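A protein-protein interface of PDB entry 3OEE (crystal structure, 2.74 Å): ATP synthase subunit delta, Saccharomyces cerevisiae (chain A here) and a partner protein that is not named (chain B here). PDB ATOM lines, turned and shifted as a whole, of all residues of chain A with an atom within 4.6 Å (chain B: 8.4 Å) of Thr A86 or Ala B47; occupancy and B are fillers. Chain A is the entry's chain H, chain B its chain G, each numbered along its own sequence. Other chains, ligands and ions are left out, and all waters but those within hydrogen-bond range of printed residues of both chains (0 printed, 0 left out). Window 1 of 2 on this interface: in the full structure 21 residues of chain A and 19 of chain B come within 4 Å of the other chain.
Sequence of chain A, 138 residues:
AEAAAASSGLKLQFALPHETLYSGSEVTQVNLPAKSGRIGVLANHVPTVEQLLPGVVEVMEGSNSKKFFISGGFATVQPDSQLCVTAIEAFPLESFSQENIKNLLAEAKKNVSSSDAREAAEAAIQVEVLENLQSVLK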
ATOM      1  N   ALA A  15      11.367  13.474 -22.264  1.00  0.00           N
ATOM      2  CA  ALA A  15      11.752  13.944 -23.611  1.00  0.00           C
ATOM      3  C   ALA A  15      13.259  14.113 -23.878  1.00  0.00           C
ATOM      4  O   ALA A  15      13.902  15.036 -23.360  1.00  0.00           O
ATOM      5  CB  ALA A  15      11.003  15.239 -23.959  1.00  0.00           C
ATOM      6  N   LEU A  52      19.151  17.885 -13.507  1.00  0.00           N
ATOM      7  CA  LEU A  52      19.421  16.451 -13.422  1.00  0.00           C
ATOM      8  C   LEU A  52      20.871  16.165 -13.809  1.00  0.00           C
ATOM      9  O   LEU A  52      21.282  16.429 -14.936  1.00  0.00           O
ATOM     10  CB  LEU A  52      18.457  15.658 -14.318  1.00  0.00           C
ATOM     11  CG  LEU A  52      16.949  15.842 -14.103  1.00  0.00           C
ATOM     12  CD1 LEU A  52      16.155  15.399 -15.318  1.00  0.00           C
ATOM     13  CD2 LEU A  52      16.474  15.110 -12.862  1.00  0.00           C
ATOM     14  N   GLY A  72      22.031  13.980 -18.441  1.00  0.00           N
ATOM     15  CA  GLY A  72      21.825  15.176 -17.626  1.00  0.00           C
ATOM     16  C   GLY A  72      20.730  16.033 -18.239  1.00  0.00           C
ATOM     17  O   GLY A  72      20.286  15.769 -19.360  1.00  0.00           O
ATOM     18  N   GLY A  73      20.289  17.060 -17.516  1.00  0.00           N
ATOM     19  CA  GLY A  73      19.239  17.934 -18.024  1.00  0.00           C
ATOM     20  C   GLY A  73      18.333  18.467 -16.938  1.00  0.00           C
ATOM     21  O   GLY A  73      18.744  18.575 -15.788  1.00  0.00           O
ATOM     22  N   PHE A  74      17.097  18.800 -17.305  1.00  0.00           N
ATOM     23  CA  PHE A  74      16.191  19.486 -16.386  1.00  0.00           C
ATOM     24  C   PHE A  74      14.904  18.742 -16.077  1.00  0.00           C
ATOM     25  O   PHE A  74      14.305  18.118 -16.952  1.00  0.00           O
ATOM     26  CB  PHE A  74      15.890  20.911 -16.874  1.00  0.00           C
ATOM     27  CG  PHE A  74      16.824  21.944 -16.311  1.00  0.00           C
ATOM     28  CD1 PHE A  74      18.010  22.262 -16.963  1.00  0.00           C
ATOM     29  CD2 PHE A  74      16.526  22.587 -15.113  1.00  0.00           C
ATOM     30  CE1 PHE A  74      18.879  23.214 -16.435  1.00  0.00           C
ATOM     31  CE2 PHE A  74      17.388  23.538 -14.580  1.00  0.00           C
ATOM     32  CZ  PHE A  74      18.567  23.850 -15.241  1.00  0.00           C
ATOM     33  N   THR A  76      11.181  19.589 -14.259  1.00  0.00           N
ATOM     34  CA  THR A  76      10.314  20.664 -13.783  1.00  0.00           C
ATOM     35  C   THR A  76       8.932  20.133 -13.376  1.00  0.00           C
ATOM     36  O   THR A  76       8.193  19.591 -14.206  1.00  0.00           O
ATOM     37  CB  THR A  76      10.174  21.833 -14.817  1.00  0.00           C
ATOM     38  OG1 THR A  76       9.034  21.616 -15.652  1.00  0.00           O
ATOM     39  CG2 THR A  76      11.422  21.982 -15.700  1.00  0.00           C
ATOM     40  N   GLN A  78       5.341  21.158 -12.587  1.00  0.00           N
ATOM     41  CA  GLN A  78       4.625  22.316 -13.133  1.00  0.00           C
ATOM     42  C   GLN A  78       3.386  22.714 -12.300  1.00  0.00           C
ATOM     43  O   GLN A  78       2.987  21.970 -11.398  1.00  0.00           O
ATOM     44  CB  GLN A  78       4.258  22.068 -14.607  1.00  0.00           C
ATOM     45  CG  GLN A  78       5.416  21.595 -15.513  1.00  0.00           C
ATOM     46  CD  GLN A  78       6.435  22.686 -15.846  1.00  0.00           C
ATOM     47  OE1 GLN A  78       7.017  23.314 -14.955  1.00  0.00           O
ATOM     48  NE2 GLN A  78       6.679  22.891 -17.139  1.00  0.00           N
ATOM     49  N   CYS A  84       7.813  17.107 -15.643  1.00  0.00           N
ATOM     50  CA  CYS A  84       8.504  17.171 -16.921  1.00  0.00           C
ATOM     51  C   CYS A  84       9.979  16.832 -16.753  1.00  0.00           C
ATOM     52  O   CYS A  84      10.697  17.494 -15.999  1.00  0.00           O
ATOM     53  CB  CYS A  84       8.330  18.547 -17.570  1.00  0.00           C
ATOM     54  SG  CYS A  84       6.637  18.888 -18.147  1.00  0.00           S
ATOM     55  N   VAL A  85      10.407  15.782 -17.452  1.00  0.00           N
ATOM     56  CA  VAL A  85      11.808  15.374 -17.509  1.00  0.00           C
ATOM     57  C   VAL A  85      12.369  15.682 -18.894  1.00  0.00           C
ATOM     58  O   VAL A  85      11.667  15.536 -19.900  1.00  0.00           O
ATOM     59  CB  VAL A  85      11.976  13.861 -17.245  1.00  0.00           C
ATOM     60  CG1 VAL A  85      13.457  13.494 -17.101  1.00  0.00           C
ATOM     61  CG2 VAL A  85      11.192  13.442 -16.012  1.00  0.00           C
ATOM     62  N   THR A  86      13.625  16.126 -18.934  1.00  0.00           N
ATOM     63  CA  THR A  86      14.384  16.271 -20.179  1.00  0.00           C
ATOM     64  C   THR A  86      15.847  15.935 -19.918  1.00  0.00           C
ATOM     65  O   THR A  86      16.482  16.539 -19.053  1.00  0.00           O
ATOM     66  CB  THR A  86      14.328  17.709 -20.765  1.00  0.00           C
ATOM     67  OG1 THR A  86      14.773  18.649 -19.779  1.00  0.00           O
ATOM     68  CG2 THR A  86      12.929  18.087 -21.242  1.00  0.00           C
ATOM     69  N   ALA A  87      16.366  14.961 -20.655  1.00  0.00           N
ATOM     70  CA  ALA A  87      17.801  14.684 -20.679  1.00  0.00           C
ATOM     71  C   ALA A  87      18.292  14.791 -22.119  1.00  0.00           C
ATOM     72  O   ALA A  87      17.557  15.260 -22.986  1.00  0.00           O
ATOM     73  CB  ALA A  87      18.094  13.312 -20.105  1.00  0.00           C
ATOM     74  N   SER B  40      10.380  15.134 -32.097  1.00  0.00           N
ATOM     75  CA  SER B  40      11.188  14.876 -30.910  1.00  0.00           C
ATOM     76  C   SER B  40      11.722  16.163 -30.270  1.00  0.00           C
ATOM     77  O   SER B  40      11.856  16.251 -29.045  1.00  0.00           O
ATOM     78  CB  SER B  40      12.335  13.921 -31.246  1.00  0.00           C
ATOM     79  OG  SER B  40      11.933  12.570 -31.110  1.00  0.00           O
ATOM     80  N   ALA B  41      12.010  17.156 -31.109  1.00  0.00           N
ATOM     81  CA  ALA B  41      12.513  18.447 -30.645  1.00  0.00           C
ATOM     82  C   ALA B  41      11.441  19.267 -29.910  1.00  0.00           C
ATOM     83  O   ALA B  41      11.647  19.671 -28.755  1.00  0.00           O
ATOM     84  CB  ALA B  41      13.107  19.242 -31.814  1.00  0.00           C
ATOM     85  N   LYS B  42      10.314  19.508 -30.591  1.00  0.00           N
ATOM     86  CA  LYS B  42       9.152  20.198 -30.012  1.00  0.00           C
ATOM     87  C   LYS B  42       8.786  19.614 -28.662  1.00  0.00           C
ATOM     88  O   LYS B  42       8.699  20.336 -27.669  1.00  0.00           O
ATOM     89  CB  LYS B  42       7.942  20.116 -30.949  1.00  0.00           C
ATOM     90  CG  LYS B  42       7.590  21.425 -31.635  1.00  0.00           C
ATOM     91  CD  LYS B  42       6.845  21.175 -32.944  1.00  0.00           C
ATOM     92  CE  LYS B  42       6.573  22.480 -33.687  1.00  0.00           C
ATOM     93  NZ  LYS B  42       6.532  22.276 -35.166  1.00  0.00           N
ATOM     94  N   LYS B  43       8.595  18.296 -28.640  1.00  0.00           N
ATOM     95  CA  LYS B  43       8.221  17.567 -27.437  1.00  0.00           C
ATOM     96  C   LYS B  43       9.155  17.881 -26.267  1.00  0.00           C
ATOM     97  O   LYS B  43       8.697  18.058 -25.142  1.00  0.00           O
ATOM     98  CB  LYS B  43       8.182  16.064 -27.726  1.00  0.00           C
ATOM     99  CG  LYS B  43       6.867  15.383 -27.350  1.00  0.00           C
ATOM    100  CD  LYS B  43       5.661  16.208 -27.800  1.00  0.00           C
ATOM    101  CE  LYS B  43       4.410  15.360 -27.924  1.00  0.00           C
ATOM    102  NZ  LYS B  43       3.184  16.205 -27.865  1.00  0.00           N
ATOM    103  N   MET B  44      10.456  17.975 -26.543  1.00  0.00           N
ATOM    104  CA  MET B  44      11.430  18.360 -25.523  1.00  0.00           C
ATOM    105  C   MET B  44      11.270  19.819 -25.098  1.00  0.00           C
ATOM    106  O   MET B  44      11.298  20.128 -23.903  1.00  0.00           O
ATOM    107  CB  MET B  44      12.856  18.106 -25.998  1.00  0.00           C
ATOM    108  CG  MET B  44      13.878  18.364 -24.925  1.00  0.00           C
ATOM    109  SD  MET B  44      15.504  17.864 -25.447  1.00  0.00           S
ATOM    110  CE  MET B  44      16.406  17.878 -23.907  1.00  0.00           C
ATOM    111  N   ASP B  45      11.096  20.703 -26.079  1.00  0.00           N
ATOM    112  CA  ASP B  45      10.892  22.137 -25.829  1.00  0.00           C
ATOM    113  C   ASP B  45       9.597  22.409 -25.063  1.00  0.00           C
ATOM    114  O   ASP B  45       9.551  23.299 -24.206  1.00  0.00           O
ATOM    115  CB  ASP B  45      10.877  22.918 -27.147  1.00  0.00           C
ATOM    116  CG  ASP B  45      11.500  24.292 -27.016  1.00  0.00           C
ATOM    117  OD1 ASP B  45      12.489  24.431 -26.257  1.00  0.00           O
ATOM    118  OD2 ASP B  45      11.012  25.232 -27.682  1.00  0.00           O
ATOM    119  N   GLU B  46       8.555  21.637 -25.378  1.00  0.00           N
ATOM    120  CA  GLU B  46       7.248  21.774 -24.735  1.00  0.00           C
ATOM    121  C   GLU B  46       7.355  21.603 -23.222  1.00  0.00           C
ATOM    122  O   GLU B  46       6.622  22.242 -22.468  1.00  0.00           O
ATOM    123  CB  GLU B  46       6.246  20.768 -25.310  1.00  0.00           C
ATOM    124  CG  GLU B  46       5.946  20.941 -26.806  1.00  0.00           C
ATOM    125  CD  GLU B  46       4.916  22.023 -27.108  1.00  0.00           C
ATOM    126  OE1 GLU B  46       3.839  22.028 -26.471  1.00  0.00           O
ATOM    127  OE2 GLU B  46       5.178  22.853 -28.005  1.00  0.00           O
ATOM    128  N   ALA B  47       8.284  20.746 -22.798  1.00  0.00           N
ATOM    129  CA  ALA B  47       8.541  20.485 -21.381  1.00  0.00           C
ATOM    130  C   ALA B  47       9.398  21.570 -20.735  1.00  0.00           C
ATOM    131  O   ALA B  47       9.401  21.718 -19.518  1.00  0.00           O
ATOM    132  CB  ALA B  47       9.209  19.119 -21.213  1.00  0.00           C
ATOM    133  N   GLU B  48      10.123  22.319 -21.562  1.00  0.00           N
ATOM    134  CA  GLU B  48      11.094  23.309 -21.090  1.00  0.00           C
ATOM    135  C   GLU B  48      10.537  24.738 -21.074  1.00  0.00           C
ATOM    136  O   GLU B  48      10.685  25.449 -20.084  1.00  0.00           O
ATOM    137  CB  GLU B  48      12.379  23.216 -21.931  1.00  0.00           C
ATOM    138  CG  GLU B  48      13.173  24.519 -22.064  1.00  0.00           C
ATOM    139  CD  GLU B  48      14.511  24.320 -22.755  1.00  0.00           C
ATOM    140  OE1 GLU B  48      15.495  23.974 -22.058  1.00  0.00           O
ATOM    141  OE2 GLU B  48      14.580  24.519 -23.989  1.00  0.00           O
ATOM    142  N   GLN B  49       9.905  25.145 -22.175  1.00  0.00           N
ATOM    143  CA  GLN B  49       9.323  26.484 -22.295  1.00  0.00           C
ATOM    144  C   GLN B  49       7.958  26.632 -21.618  1.00  0.00           C
ATOM    145  O   GLN B  49       7.380  27.727 -21.601  1.00  0.00           O
ATOM    146  CB  GLN B  49       9.247  26.926 -23.759  1.00  0.00           C
ATOM    147  CG  GLN B  49      10.495  27.639 -24.236  1.00  0.00           C
ATOM    148  CD  GLN B  49      10.208  28.681 -25.307  1.00  0.00           C
ATOM    149  OE1 GLN B  49       9.774  28.351 -26.415  1.00  0.00           O
ATOM    150  NE2 GLN B  49      10.467  29.949 -24.985  1.00  0.00           N
ATOM    151  N   LEU B  50       7.445  25.536 -21.061  1.00  0.00           N
ATOM    152  CA  LEU B  50       6.200  25.591 -20.301  1.00  0.00           C
ATOM    153  C   LEU B  50       6.426  26.283 -18.951  1.00  0.00           C
ATOM    154  O   LEU B  50       5.524  26.935 -18.420  1.00  0.00           O
ATOM    155  CB  LEU B  50       5.611  24.193 -20.111  1.00  0.00           C
ATOM    156  CG  LEU B  50       4.086  24.116 -19.984  1.00  0.00           C
ATOM    157  CD1 LEU B  50       3.405  24.266 -21.348  1.00  0.00           C
ATOM    158  CD2 LEU B  50       3.661  22.816 -19.312  1.00  0.00           C
ATOM    159  N   PHE B  51       7.637  26.138 -18.415  1.00  0.00           N
ATOM    160  CA  PHE B  51       8.057  26.820 -17.192  1.00  0.00           C
ATOM    161  C   PHE B  51       8.100  28.340 -17.381  1.00  0.00           C
ATOM    162  O   PHE B  51       7.700  29.097 -16.487  1.00  0.00           O
ATOM    163  CB  PHE B  51       9.421  26.288 -16.734  1.00  0.00           C
ATOM    164  CG  PHE B  51      10.184  27.239 -15.866  1.00  0.00           C
ATOM    165  CD1 PHE B  51      10.108  27.151 -14.485  1.00  0.00           C
ATOM    166  CD2 PHE B  51      10.983  28.226 -16.433  1.00  0.00           C
ATOM    167  CE1 PHE B  51      10.815  28.034 -13.673  1.00  0.00           C
ATOM    168  CE2 PHE B  51      11.686  29.116 -15.637  1.00  0.00           C
ATOM    169  CZ  PHE B  51      11.605  29.019 -14.251  1.00  0.00           C
ATOM    170  N   TYR B  52       8.589  28.777 -18.540  1.00  0.00           N
ATOM    171  CA  TYR B  52       8.679  30.203 -18.862  1.00  0.00           C
ATOM    172  C   TYR B  52       7.294  30.849 -18.999  1.00  0.00           C
ATOM    173  O   TYR B  52       7.113  32.022 -18.655  1.00  0.00           O
ATOM    174  CB  TYR B  52       9.489  30.414 -20.140  1.00  0.00           C
ATOM    175  CG  TYR B  52      10.960  30.045 -20.041  1.00  0.00           C
ATOM    176  CD1 TYR B  52      11.429  28.827 -20.538  1.00  0.00           C
ATOM    177  CD2 TYR B  52      11.883  30.923 -19.473  1.00  0.00           C
ATOM    178  CE1 TYR B  52      12.776  28.490 -20.463  1.00  0.00           C
ATOM    179  CE2 TYR B  52      13.235  30.594 -19.396  1.00  0.00           C
ATOM    180  CZ  TYR B  52      13.673  29.377 -19.893  1.00  0.00           C
ATOM    181  OH  TYR B  52      15.008  29.045 -19.817  1.00  0.00           O
ATOM    182  N   ASN B  54       4.642  29.927 -17.235  1.00  0.00           N
ATOM    183  CA  ASN B  54       4.092  30.050 -15.888  1.00  0.00           C
ATOM    184  C   ASN B  54       4.720  31.193 -15.106  1.00  0.00           C
ATOM    185  O   ASN B  54       4.026  31.938 -14.411  1.00  0.00           O
ATOM    186  CB  ASN B  54       4.262  28.745 -15.117  1.00  0.00           C
ATOM    187  CG  ASN B  54       3.593  27.576 -15.796  1.00  0.00           C
ATOM    188  OD1 ASN B  54       2.438  27.655 -16.218  1.00  0.00           O
ATOM    189  ND2 ASN B  54       4.313  26.472 -15.898  1.00  0.00           N
ATOM    190  N   LEU B 209      19.612  26.861 -16.531  1.00  0.00           N
ATOM    191  CA  LEU B 209      18.356  26.841 -17.288  1.00  0.00           C
ATOM    192  C   LEU B 209      18.399  27.763 -18.510  1.00  0.00           C
ATOM    193  O   LEU B 209      17.675  27.551 -19.472  1.00  0.00           O
ATOM    194  CB  LEU B 209      17.163  27.178 -16.387  1.00  0.00           C
ATOM    195  CG  LEU B 209      15.736  27.107 -16.953  1.00  0.00           C
ATOM    196  CD1 LEU B 209      15.471  25.832 -17.756  1.00  0.00           C
ATOM    197  CD2 LEU B 209      14.733  27.238 -15.818  1.00  0.00           C
ATOM    198  N   TYR B 212      21.205  25.722 -20.891  1.00  0.00           N
ATOM    199  CA  TYR B 212      20.518  24.525 -21.354  1.00  0.00           C
ATOM    200  C   TYR B 212      19.430  24.872 -22.365  1.00  0.00           C
ATOM    201  O   TYR B 212      19.211  24.137 -23.322  1.00  0.00           O
ATOM    202  CB  TYR B 212      19.913  23.815 -20.143  1.00  0.00           C
ATOM    203  CG  TYR B 212      19.164  22.538 -20.428  1.00  0.00           C
ATOM    204  CD1 TYR B 212      19.841  21.333 -20.587  1.00  0.00           C
ATOM    205  CD2 TYR B 212      17.772  22.531 -20.496  1.00  0.00           C
ATOM    206  CE1 TYR B 212      19.155  20.160 -20.835  1.00  0.00           C
ATOM    207  CE2 TYR B 212      17.075  21.363 -20.739  1.00  0.00           C
ATOM    208  CZ  TYR B 212      17.772  20.184 -20.907  1.00  0.00           C
ATOM    209  OH  TYR B 212      17.088  19.020 -21.146  1.00  0.00           O
ATOM    210  N   ASN B 216      18.869  24.058 -26.388  1.00  0.00           N
ATOM    211  CA  ASN B 216      17.600  23.430 -26.754  1.00  0.00           C
ATOM    212  C   ASN B 216      16.709  24.206 -27.714  1.00  0.00           C
ATOM    213  O   ASN B 216      16.229  23.653 -28.707  1.00  0.00           O
ATOM    214  CB  ASN B 216      16.796  23.126 -25.496  1.00  0.00           C
ATOM    215  CG  ASN B 216      17.050  21.746 -24.956  1.00  0.00           C
ATOM    216  OD1 ASN B 216      16.138  21.118 -24.424  1.00  0.00           O
ATOM    217  ND2 ASN B 216      18.284  21.264 -25.075  1.00  0.00           N
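Of the 17 printed residues of chain B, 7 touch a printed residue of chain A.
Printed residues of chain B that touch a printed residue of chain A: Lys B43, Met B44, Ala B47, Leu B50, Phe B51, Leu B209 and Tyr B212.
Hydrophobic or aromatic side chains of chain B within 4 Å of the printed part of chain A: Met B44, Ala B47, Leu B50, Leu B209 and Tyr B212.
Hydrophobic or aromatic side chains of chain A within 4 Å of the printed part of chain B: Ala A15 and Phe A74.
Among the printed residues, no Asp or Glu carboxylate lies within 4 Å of a Lys or Arg side-chain nitrogen of the other chain.
Thr A86 touches just these residues of chain B: Met B44, Ala B47 and Tyr B212.
Ala B47 touches four residues of chain A.
Ala A87 touches just one residue of chain B: Met B44 (3.0 Å).
Of the printed residues of chain A, Leu B50 touches Gln A78.
Printed residues of chain B within 4 Å of Gly A73: Tyr B212 (3.6 Å).
Printed residues of chain A within 4 Å of Leu B209: Phe A74 (3.4 Å).
The nearest residue of chain A that does not touch Ala B47 is Val A85 (4.5 Å).
Among the printed residues, pairs that only touch across the chains: Ala A87 with Met B44 (3.0 Å), Gln A78 with Leu B50 (3.4 Å), Phe A74 with Leu B209 (3.4 Å), Ala A15 with Met B44 (3.5 Å), Phe A74 with Tyr B212 (3.6 Å), Gly A73 with Tyr B212 (3.6 Å), Gln A78 with Phe B51 (3.6 Å), Thr A86 with Met B44 (3.7 Å), Cys A84 with Ala B47 (3.8 Å), Gln A78 with Ala B47 (3.8 Å), Ala A15 with Lys B43 (3.8 Å), Thr A86 with Ala B47 (3.9 Å) and Thr A76 with Ala B47 (3.9 Å).
The backbone NH (N) of Ala A15 lies within hydrogen-bond range of the backbone carbonyl oxygen (O) of Val A85, at 3.2 Å.
OG1 of Thr A76 sits at hydrogen-bond distance from OE1 of Gln A78 (2.7 Å).
The side-chain hydroxyl (OH) of Tyr B52 is in hydrogen-bond range of the backbone carbonyl oxygen (O) of Leu B209 (3.1 Å).
N of Thr A76 lies within hydrogen-bond range of O of Cys A84 (2.8 Å).
O of Leu B50 lies within hydrogen-bond range of ND2 of Asn B54.
The side-chain amide oxygen (OD1) of Asn B216 sits close to the side-chain sulfur (SD) of Met B44, 3.5 Å away.
The side-chain hydroxyl of Tyr B212 sits at hydrogen-bond distance from the side-chain hydroxyl of Thr A86, 2.7 Å away.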
